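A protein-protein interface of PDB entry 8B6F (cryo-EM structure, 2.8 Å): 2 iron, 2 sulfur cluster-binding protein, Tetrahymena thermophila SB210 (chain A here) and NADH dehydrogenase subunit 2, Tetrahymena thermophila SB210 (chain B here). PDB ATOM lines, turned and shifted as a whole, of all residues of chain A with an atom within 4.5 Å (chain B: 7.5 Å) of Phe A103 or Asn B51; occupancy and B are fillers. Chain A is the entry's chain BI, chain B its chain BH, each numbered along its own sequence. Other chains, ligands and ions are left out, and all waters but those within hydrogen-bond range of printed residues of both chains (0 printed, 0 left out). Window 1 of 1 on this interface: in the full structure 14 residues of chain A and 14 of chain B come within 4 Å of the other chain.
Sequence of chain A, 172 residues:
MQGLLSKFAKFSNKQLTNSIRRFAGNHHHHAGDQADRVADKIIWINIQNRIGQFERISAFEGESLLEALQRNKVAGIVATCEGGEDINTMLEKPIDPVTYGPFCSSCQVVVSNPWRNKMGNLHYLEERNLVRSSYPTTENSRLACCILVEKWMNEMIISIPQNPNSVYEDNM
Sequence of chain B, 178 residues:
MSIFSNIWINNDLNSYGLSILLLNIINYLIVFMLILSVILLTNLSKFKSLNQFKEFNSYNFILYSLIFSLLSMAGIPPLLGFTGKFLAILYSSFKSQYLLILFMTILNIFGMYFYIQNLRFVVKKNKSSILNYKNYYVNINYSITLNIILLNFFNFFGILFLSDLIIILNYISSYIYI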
ATOM      1  N   CYS A  81      -0.287  30.537   3.805  1.00  0.00           N
ATOM      2  CA  CYS A  81       0.135  30.745   5.182  1.00  0.00           C
ATOM      3  C   CYS A  81      -0.057  32.177   5.661  1.00  0.00           C
ATOM      4  O   CYS A  81      -0.005  32.422   6.871  1.00  0.00           O
ATOM      5  CB  CYS A  81       1.607  30.335   5.285  1.00  0.00           C
ATOM      6  SG  CYS A  81       2.772  31.684   4.956  1.00  0.00           S
ATOM      7  N   GLY A  84       3.277  33.798   7.354  1.00  0.00           N
ATOM      8  CA  GLY A  84       4.039  32.948   8.248  1.00  0.00           C
ATOM      9  C   GLY A  84       3.820  33.294   9.710  1.00  0.00           C
ATOM     10  O   GLY A  84       2.797  33.857  10.111  1.00  0.00           O
ATOM     11  N   GLU A  85       4.815  32.940  10.520  1.00  0.00           N
ATOM     12  CA  GLU A  85       4.729  33.115  11.962  1.00  0.00           C
ATOM     13  C   GLU A  85       4.816  34.590  12.338  1.00  0.00           C
ATOM     14  O   GLU A  85       5.346  35.412  11.588  1.00  0.00           O
ATOM     15  CB  GLU A  85       5.844  32.340  12.660  1.00  0.00           C
ATOM     16  CG  GLU A  85       5.591  32.102  14.137  1.00  0.00           C
ATOM     17  CD  GLU A  85       6.766  31.445  14.826  1.00  0.00           C
ATOM     18  OE1 GLU A  85       7.847  31.366  14.209  1.00  0.00           O
ATOM     19  OE2 GLU A  85       6.611  31.008  15.985  1.00  0.00           O
ATOM     20  N   TYR A 100      11.303  29.426  12.003  1.00  0.00           N
ATOM     21  CA  TYR A 100      10.784  28.299  11.241  1.00  0.00           C
ATOM     22  C   TYR A 100      10.680  28.586   9.750  1.00  0.00           C
ATOM     23  O   TYR A 100      10.405  27.664   8.976  1.00  0.00           O
ATOM     24  CB  TYR A 100       9.407  27.889  11.771  1.00  0.00           C
ATOM     25  CG  TYR A 100       9.465  26.946  12.947  1.00  0.00           C
ATOM     26  CD1 TYR A 100       9.745  27.411  14.223  1.00  0.00           C
ATOM     27  CD2 TYR A 100       9.238  25.587  12.781  1.00  0.00           C
ATOM     28  CE1 TYR A 100       9.801  26.552  15.300  1.00  0.00           C
ATOM     29  CE2 TYR A 100       9.292  24.719  13.849  1.00  0.00           C
ATOM     30  CZ  TYR A 100       9.574  25.206  15.107  1.00  0.00           C
ATOM     31  OH  TYR A 100       9.627  24.345  16.178  1.00  0.00           O
ATOM     32  N   GLY A 101      10.885  29.830   9.331  1.00  0.00           N
ATOM     33  CA  GLY A 101      10.840  30.180   7.934  1.00  0.00           C
ATOM     34  C   GLY A 101       9.423  30.206   7.411  1.00  0.00           C
ATOM     35  O   GLY A 101       8.455  30.080   8.165  1.00  0.00           O
ATOM     36  N   PRO A 102       9.271  30.375   6.101  1.00  0.00           N
ATOM     37  CA  PRO A 102       7.929  30.358   5.516  1.00  0.00           C
ATOM     38  C   PRO A 102       7.279  28.992   5.669  1.00  0.00           C
ATOM     39  O   PRO A 102       7.945  27.956   5.674  1.00  0.00           O
ATOM     40  CB  PRO A 102       8.174  30.703   4.043  1.00  0.00           C
ATOM     41  CG  PRO A 102       9.588  30.338   3.798  1.00  0.00           C
ATOM     42  CD  PRO A 102      10.317  30.568   5.083  1.00  0.00           C
ATOM     43  N   PHE A 103       5.957  29.007   5.797  1.00  0.00           N
ATOM     44  CA  PHE A 103       5.171  27.801   6.002  1.00  0.00           C
ATOM     45  C   PHE A 103       4.534  27.301   4.718  1.00  0.00           C
ATOM     46  O   PHE A 103       3.769  26.334   4.756  1.00  0.00           O
ATOM     47  CB  PHE A 103       4.098  28.041   7.063  1.00  0.00           C
ATOM     48  CG  PHE A 103       4.626  27.995   8.461  1.00  0.00           C
ATOM     49  CD1 PHE A 103       5.369  29.046   8.969  1.00  0.00           C
ATOM     50  CD2 PHE A 103       4.392  26.893   9.265  1.00  0.00           C
ATOM     51  CE1 PHE A 103       5.861  29.004  10.253  1.00  0.00           C
ATOM     52  CE2 PHE A 103       4.883  26.845  10.552  1.00  0.00           C
ATOM     53  CZ  PHE A 103       5.620  27.901  11.046  1.00  0.00           C
ATOM     54  N   CYS A 104       4.831  27.931   3.591  1.00  0.00           N
ATOM     55  CA  CYS A 104       4.409  27.437   2.286  1.00  0.00           C
ATOM     56  C   CYS A 104       5.122  28.230   1.203  1.00  0.00           C
ATOM     57  O   CYS A 104       6.002  29.049   1.483  1.00  0.00           O
ATOM     58  CB  CYS A 104       2.897  27.616   2.157  1.00  0.00           C
ATOM     59  SG  CYS A 104       2.467  29.369   1.767  1.00  0.00           S
ATOM     60  N   ASN A 129      11.571  26.049   0.514  1.00  0.00           N
ATOM     61  CA  ASN A 129      10.175  26.202   0.119  1.00  0.00           C
ATOM     62  C   ASN A 129      10.049  26.456  -1.378  1.00  0.00           C
ATOM     63  O   ASN A 129       9.170  25.892  -2.038  1.00  0.00           O
ATOM     64  CB  ASN A 129       9.531  27.333   0.916  1.00  0.00           C
ATOM     65  CG  ASN A 129       9.323  26.967   2.370  1.00  0.00           C
ATOM     66  OD1 ASN A 129       8.218  26.623   2.783  1.00  0.00           O
ATOM     67  ND2 ASN A 129      10.393  27.027   3.154  1.00  0.00           N
ATOM     68  N   LYS B  46     -10.053  29.716   7.967  1.00  0.00           N
ATOM     69  CA  LYS B  46      -8.864  30.378   8.494  1.00  0.00           C
ATOM     70  C   LYS B  46      -7.721  29.394   8.706  1.00  0.00           C
ATOM     71  O   LYS B  46      -6.552  29.744   8.510  1.00  0.00           O
ATOM     72  CB  LYS B  46      -9.202  31.088   9.804  1.00  0.00           C
ATOM     73  CG  LYS B  46     -10.204  32.220   9.658  1.00  0.00           C
ATOM     74  CD  LYS B  46      -9.614  33.382   8.878  1.00  0.00           C
ATOM     75  CE  LYS B  46     -10.566  34.565   8.850  1.00  0.00           C
ATOM     76  NZ  LYS B  46      -9.984  35.726   8.122  1.00  0.00           N
ATOM     77  N   LYS B  48      -5.460  26.689   7.703  1.00  0.00           N
ATOM     78  CA  LYS B  48      -4.942  25.937   6.569  1.00  0.00           C
ATOM     79  C   LYS B  48      -3.447  25.658   6.651  1.00  0.00           C
ATOM     80  O   LYS B  48      -2.918  24.996   5.755  1.00  0.00           O
ATOM     81  CB  LYS B  48      -5.253  26.672   5.256  1.00  0.00           C
ATOM     82  CG  LYS B  48      -4.689  28.077   5.183  1.00  0.00           C
ATOM     83  CD  LYS B  48      -5.257  28.841   3.999  1.00  0.00           C
ATOM     84  CE  LYS B  48      -6.678  29.301   4.261  1.00  0.00           C
ATOM     85  NZ  LYS B  48      -7.194  30.134   3.140  1.00  0.00           N
ATOM     86  N   SER B  49      -2.752  26.130   7.684  1.00  0.00           N
ATOM     87  CA  SER B  49      -1.333  25.848   7.846  1.00  0.00           C
ATOM     88  C   SER B  49      -1.002  25.817   9.329  1.00  0.00           C
ATOM     89  O   SER B  49      -1.710  26.399  10.153  1.00  0.00           O
ATOM     90  CB  SER B  49      -0.462  26.889   7.135  1.00  0.00           C
ATOM     91  OG  SER B  49      -0.635  26.831   5.732  1.00  0.00           O
ATOM     92  N   LEU B  50       0.094  25.131   9.662  1.00  0.00           N
ATOM     93  CA  LEU B  50       0.534  25.094  11.052  1.00  0.00           C
ATOM     94  C   LEU B  50       0.764  26.495  11.588  1.00  0.00           C
ATOM     95  O   LEU B  50       0.534  26.755  12.775  1.00  0.00           O
ATOM     96  CB  LEU B  50       1.811  24.267  11.186  1.00  0.00           C
ATOM     97  CG  LEU B  50       1.731  22.810  10.735  1.00  0.00           C
ATOM     98  CD1 LEU B  50       3.033  22.104  11.053  1.00  0.00           C
ATOM     99  CD2 LEU B  50       0.560  22.088  11.377  1.00  0.00           C
ATOM    100  N   ASN B  51       1.221  27.407  10.731  1.00  0.00           N
ATOM    101  CA  ASN B  51       1.333  28.803  11.123  1.00  0.00           C
ATOM    102  C   ASN B  51      -0.006  29.357  11.587  1.00  0.00           C
ATOM    103  O   ASN B  51      -0.050  30.203  12.486  1.00  0.00           O
ATOM    104  CB  ASN B  51       1.864  29.616   9.945  1.00  0.00           C
ATOM    105  CG  ASN B  51       1.611  31.091  10.096  1.00  0.00           C
ATOM    106  OD1 ASN B  51       1.746  31.645  11.184  1.00  0.00           O
ATOM    107  ND2 ASN B  51       1.232  31.741   9.002  1.00  0.00           N
ATOM    108  N   GLN B  52      -1.104  28.882  11.001  1.00  0.00           N
ATOM    109  CA  GLN B  52      -2.428  29.398  11.317  1.00  0.00           C
ATOM    110  C   GLN B  52      -2.908  28.998  12.702  1.00  0.00           C
ATOM    111  O   GLN B  52      -4.031  29.358  13.068  1.00  0.00           O
ATOM    112  CB  GLN B  52      -3.435  28.925  10.269  1.00  0.00           C
ATOM    113  CG  GLN B  52      -3.045  29.250   8.833  1.00  0.00           C
ATOM    114  CD  GLN B  52      -3.076  30.731   8.534  1.00  0.00           C
ATOM    115  OE1 GLN B  52      -3.341  31.550   9.410  1.00  0.00           O
ATOM    116  NE2 GLN B  52      -2.813  31.081   7.283  1.00  0.00           N
ATOM    117  N   PHE B  53      -2.112  28.258  13.476  1.00  0.00           N
ATOM    118  CA  PHE B  53      -2.472  28.018  14.868  1.00  0.00           C
ATOM    119  C   PHE B  53      -2.610  29.326  15.632  1.00  0.00           C
ATOM    120  O   PHE B  53      -3.331  29.389  16.631  1.00  0.00           O
ATOM    121  CB  PHE B  53      -1.433  27.121  15.541  1.00  0.00           C
ATOM    122  CG  PHE B  53      -1.811  25.671  15.560  1.00  0.00           C
ATOM    123  CD1 PHE B  53      -2.687  25.187  16.515  1.00  0.00           C
ATOM    124  CD2 PHE B  53      -1.285  24.790  14.632  1.00  0.00           C
ATOM    125  CE1 PHE B  53      -3.038  23.853  16.540  1.00  0.00           C
ATOM    126  CE2 PHE B  53      -1.630  23.453  14.653  1.00  0.00           C
ATOM    127  CZ  PHE B  53      -2.509  22.986  15.608  1.00  0.00           C
ATOM    128  N   LYS B  54      -1.926  30.377  15.177  1.00  0.00           N
ATOM    129  CA  LYS B  54      -2.105  31.691  15.781  1.00  0.00           C
ATOM    130  C   LYS B  54      -3.551  32.151  15.685  1.00  0.00           C
ATOM    131  O   LYS B  54      -4.019  32.912  16.540  1.00  0.00           O
ATOM    132  CB  LYS B  54      -1.181  32.708  15.110  1.00  0.00           C
ATOM    133  CG  LYS B  54      -1.470  32.933  13.636  1.00  0.00           C
ATOM    134  CD  LYS B  54      -0.469  33.896  13.024  1.00  0.00           C
ATOM    135  CE  LYS B  54      -0.685  34.035  11.529  1.00  0.00           C
ATOM    136  NZ  LYS B  54       0.285  34.982  10.916  1.00  0.00           N
ATOM    137  N   GLU B  55      -4.276  31.704  14.657  1.00  0.00           N
ATOM    138  CA  GLU B  55      -5.675  32.084  14.519  1.00  0.00           C
ATOM    139  C   GLU B  55      -6.513  31.617  15.698  1.00  0.00           C
ATOM    140  O   GLU B  55      -7.565  32.207  15.966  1.00  0.00           O
ATOM    141  CB  GLU B  55      -6.247  31.514  13.221  1.00  0.00           C
ATOM    142  CG  GLU B  55      -5.542  32.008  11.971  1.00  0.00           C
ATOM    143  CD  GLU B  55      -5.684  33.503  11.771  1.00  0.00           C
ATOM    144  OE1 GLU B  55      -6.526  34.120  12.453  1.00  0.00           O
ATOM    145  OE2 GLU B  55      -4.952  34.062  10.927  1.00  0.00           O
ATOM    146  N   PHE B  56      -6.074  30.584  16.411  1.00  0.00           N
ATOM    147  CA  PHE B  56      -6.740  30.198  17.647  1.00  0.00           C
ATOM    148  C   PHE B  56      -6.545  31.217  18.757  1.00  0.00           C
ATOM    149  O   PHE B  56      -7.195  31.103  19.800  1.00  0.00           O
ATOM    150  CB  PHE B  56      -6.232  28.842  18.125  1.00  0.00           C
ATOM    151  CG  PHE B  56      -6.763  27.678  17.342  1.00  0.00           C
ATOM    152  CD1 PHE B  56      -8.092  27.305  17.448  1.00  0.00           C
ATOM    153  CD2 PHE B  56      -5.927  26.939  16.524  1.00  0.00           C
ATOM    154  CE1 PHE B  56      -8.582  26.229  16.737  1.00  0.00           C
ATOM    155  CE2 PHE B  56      -6.410  25.861  15.809  1.00  0.00           C
ATOM    156  CZ  PHE B  56      -7.739  25.505  15.917  1.00  0.00           C
ATOM    157  N   GLN B 117       5.121  21.720  19.515  1.00  0.00           N
ATOM    158  CA  GLN B 117       5.712  22.797  18.726  1.00  0.00           C
ATOM    159  C   GLN B 117       4.657  23.778  18.229  1.00  0.00           C
ATOM    160  O   GLN B 117       4.968  24.947  17.980  1.00  0.00           O
ATOM    161  CB  GLN B 117       6.500  22.225  17.547  1.00  0.00           C
ATOM    162  CG  GLN B 117       5.657  21.502  16.515  1.00  0.00           C
ATOM    163  CD  GLN B 117       6.448  21.150  15.276  1.00  0.00           C
ATOM    164  OE1 GLN B 117       7.630  21.467  15.170  1.00  0.00           O
ATOM    165  NE2 GLN B 117       5.795  20.492  14.326  1.00  0.00           N
ATOM    166  N   ASN B 118       3.410  23.328  18.087  1.00  0.00           N
ATOM    167  CA  ASN B 118       2.349  24.214  17.624  1.00  0.00           C
ATOM    168  C   ASN B 118       1.994  25.283  18.646  1.00  0.00           C
ATOM    169  O   ASN B 118       1.453  26.326  18.267  1.00  0.00           O
ATOM    170  CB  ASN B 118       1.106  23.399  17.279  1.00  0.00           C
ATOM    171  CG  ASN B 118       1.358  22.408  16.167  1.00  0.00           C
ATOM    172  OD1 ASN B 118       2.115  22.680  15.239  1.00  0.00           O
ATOM    173  ND2 ASN B 118       0.728  21.246  16.258  1.00  0.00           N
ATOM    174  N   ARG B 120       4.061  27.143  19.990  1.00  0.00           N
ATOM    175  CA  ARG B 120       4.861  28.283  19.556  1.00  0.00           C
ATOM    176  C   ARG B 120       4.111  29.114  18.526  1.00  0.00           C
ATOM    177  O   ARG B 120       4.124  30.349  18.583  1.00  0.00           O
ATOM    178  CB  ARG B 120       6.191  27.795  18.984  1.00  0.00           C
ATOM    179  CG  ARG B 120       7.153  28.902  18.600  1.00  0.00           C
ATOM    180  CD  ARG B 120       8.441  28.319  18.047  1.00  0.00           C
ATOM    181  NE  ARG B 120       9.521  29.300  18.021  1.00  0.00           N
ATOM    182  CZ  ARG B 120       9.806  30.084  16.991  1.00  0.00           C
ATOM    183  NH1 ARG B 120       9.112  30.034  15.869  1.00  0.00           N
ATOM    184  NH2 ARG B 120      10.817  30.942  17.089  1.00  0.00           N
ATOM    185  N   PHE B 121       3.449  28.454  17.575  1.00  0.00           N
ATOM    186  CA  PHE B 121       2.710  29.178  16.549  1.00  0.00           C
ATOM    187  C   PHE B 121       1.435  29.799  17.105  1.00  0.00           C
ATOM    188  O   PHE B 121       0.942  30.789  16.556  1.00  0.00           O
ATOM    189  CB  PHE B 121       2.372  28.238  15.392  1.00  0.00           C
ATOM    190  CG  PHE B 121       3.540  27.421  14.916  1.00  0.00           C
ATOM    191  CD1 PHE B 121       4.820  27.947  14.917  1.00  0.00           C
ATOM    192  CD2 PHE B 121       3.355  26.122  14.476  1.00  0.00           C
ATOM    193  CE1 PHE B 121       5.892  27.194  14.484  1.00  0.00           C
ATOM    194  CE2 PHE B 121       4.424  25.365  14.041  1.00  0.00           C
ATOM    195  CZ  PHE B 121       5.693  25.902  14.045  1.00  0.00           C
ATOM    196  N   VAL B 122       0.887  29.236  18.184  1.00  0.00           N
ATOM    197  CA  VAL B 122      -0.344  29.770  18.761  1.00  0.00           C
ATOM    198  C   VAL B 122      -0.178  31.234  19.141  1.00  0.00           C
ATOM    199  O   VAL B 122      -1.153  31.994  19.151  1.00  0.00           O
ATOM    200  CB  VAL B 122      -0.776  28.917  19.972  1.00  0.00           C
ATOM    201  CG1 VAL B 122      -1.811  29.650  20.820  1.00  0.00           C
ATOM    202  CG2 VAL B 122      -1.332  27.582  19.509  1.00  0.00           C
ATOM    203  N   VAL B 123       1.044  31.659  19.467  1.00  0.00           N
ATOM    204  CA  VAL B 123       1.267  33.052  19.827  1.00  0.00           C
ATOM    205  C   VAL B 123       0.985  33.933  18.622  1.00  0.00           C
ATOM    206  O   VAL B 123       1.451  33.662  17.509  1.00  0.00           O
ATOM    207  CB  VAL B 123       2.700  33.249  20.344  1.00  0.00           C
ATOM    208  CG1 VAL B 123       2.964  34.714  20.657  1.00  0.00           C
ATOM    209  CG2 VAL B 123       2.949  32.388  21.570  1.00  0.00           C
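The backbone carbonyl oxygen of Gly A84 sits close to the side-chain amide oxygen of Asn B51 (2.7 Å).
O of Gly A84 is in hydrogen-bond range of NZ of Lys B54 (2.9 Å).
ND2 of Asn B51 is in hydrogen-bond range of O of Cys A81, 2.6 Å away.
The side-chain carboxylate (OE1) of Glu A85 lies within salt-bridge range of the guanidinium group (NH1) of Arg B120, 2.5 Å away.
O of Cys A81 lies within hydrogen-bond range of NE2 of Gln B52.
OD1 of Asn B51 is in hydrogen-bond range of N of Glu A85, 3.4 Å away.
OE2 of Glu B55 sits close to OE1 of Gln B52 (3.3 Å).
The backbone NH (N) of Lys B54 sits close to the backbone carbonyl oxygen (O) of Phe B121, at 3.2 Å.
The side-chain sulfur (SG) of Cys A81 sits close to the backbone NH (N) of Gly A84.
CD1 of Phe B121 touches OE2 of Glu A85 (3.7 Å).
Tyr A100 touches Gln B117.
Tyr A100 touches Arg B120 (CD1 to NH1, 3.2 Å).
Phe B121 touches Tyr A100 (CZ to CD2, 3.8 Å).
CG of Phe A103 touches CB of Asn B51, at 3.5 Å.
Phe A103 touches Phe B121 (CZ to CE1, 3.5 Å).
Of chain B, only Asn B51 (3.5 Å) and Phe B121 (3.5 Å) come within 4 Å of Phe A103.
Asn B51 touches just these residues of chain A: Cys A81 (2.6 Å), Gly A84 (2.7 Å), Glu A85 (3.4 Å) and Phe A103 (3.5 Å).
Of chain B, only Asn B51 and Lys B54 come within 4 Å of Gly A84.
Of the printed residues of chain B, Cys A81 touches Asn B51 and Gln B52.
Of the printed residues of chain A, Lys B54 touches Gly A84.
Of the printed residues of chain A, Gln B117 touches Tyr A100.
Of the printed residues of chain A, Arg B120 touches Glu A85 and Tyr A100.
Printed residues of chain B within 4 Å of Tyr A100: Gln B117, Arg B120 and Phe B121.
Val B123 touches none of the printed residues of chain A.
The nearest printed residue of chain A that does not touch Asn B51 is Gly A101 (6.8 Å).
The nearest printed residue of chain A that does not touch Gln B52 is Phe A103 (6.1 Å).
Hydrophobic or aromatic side chains of chain A that line the printed part of chain B: Tyr A100 and Phe A103.
Hydrophobic or aromatic side chains of chain B that line the printed part of chain A: Phe B121.
Along chain B the printed residues that touch a printed residue of chain A span positions 51 to 121.
Among the printed residues, 12 pairs touch across the chains.
Among the printed residues, Asp or Glu carboxylates within 4 Å of a Lys or Arg side-chain nitrogen of the other chain: Glu A85 with Arg B120.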
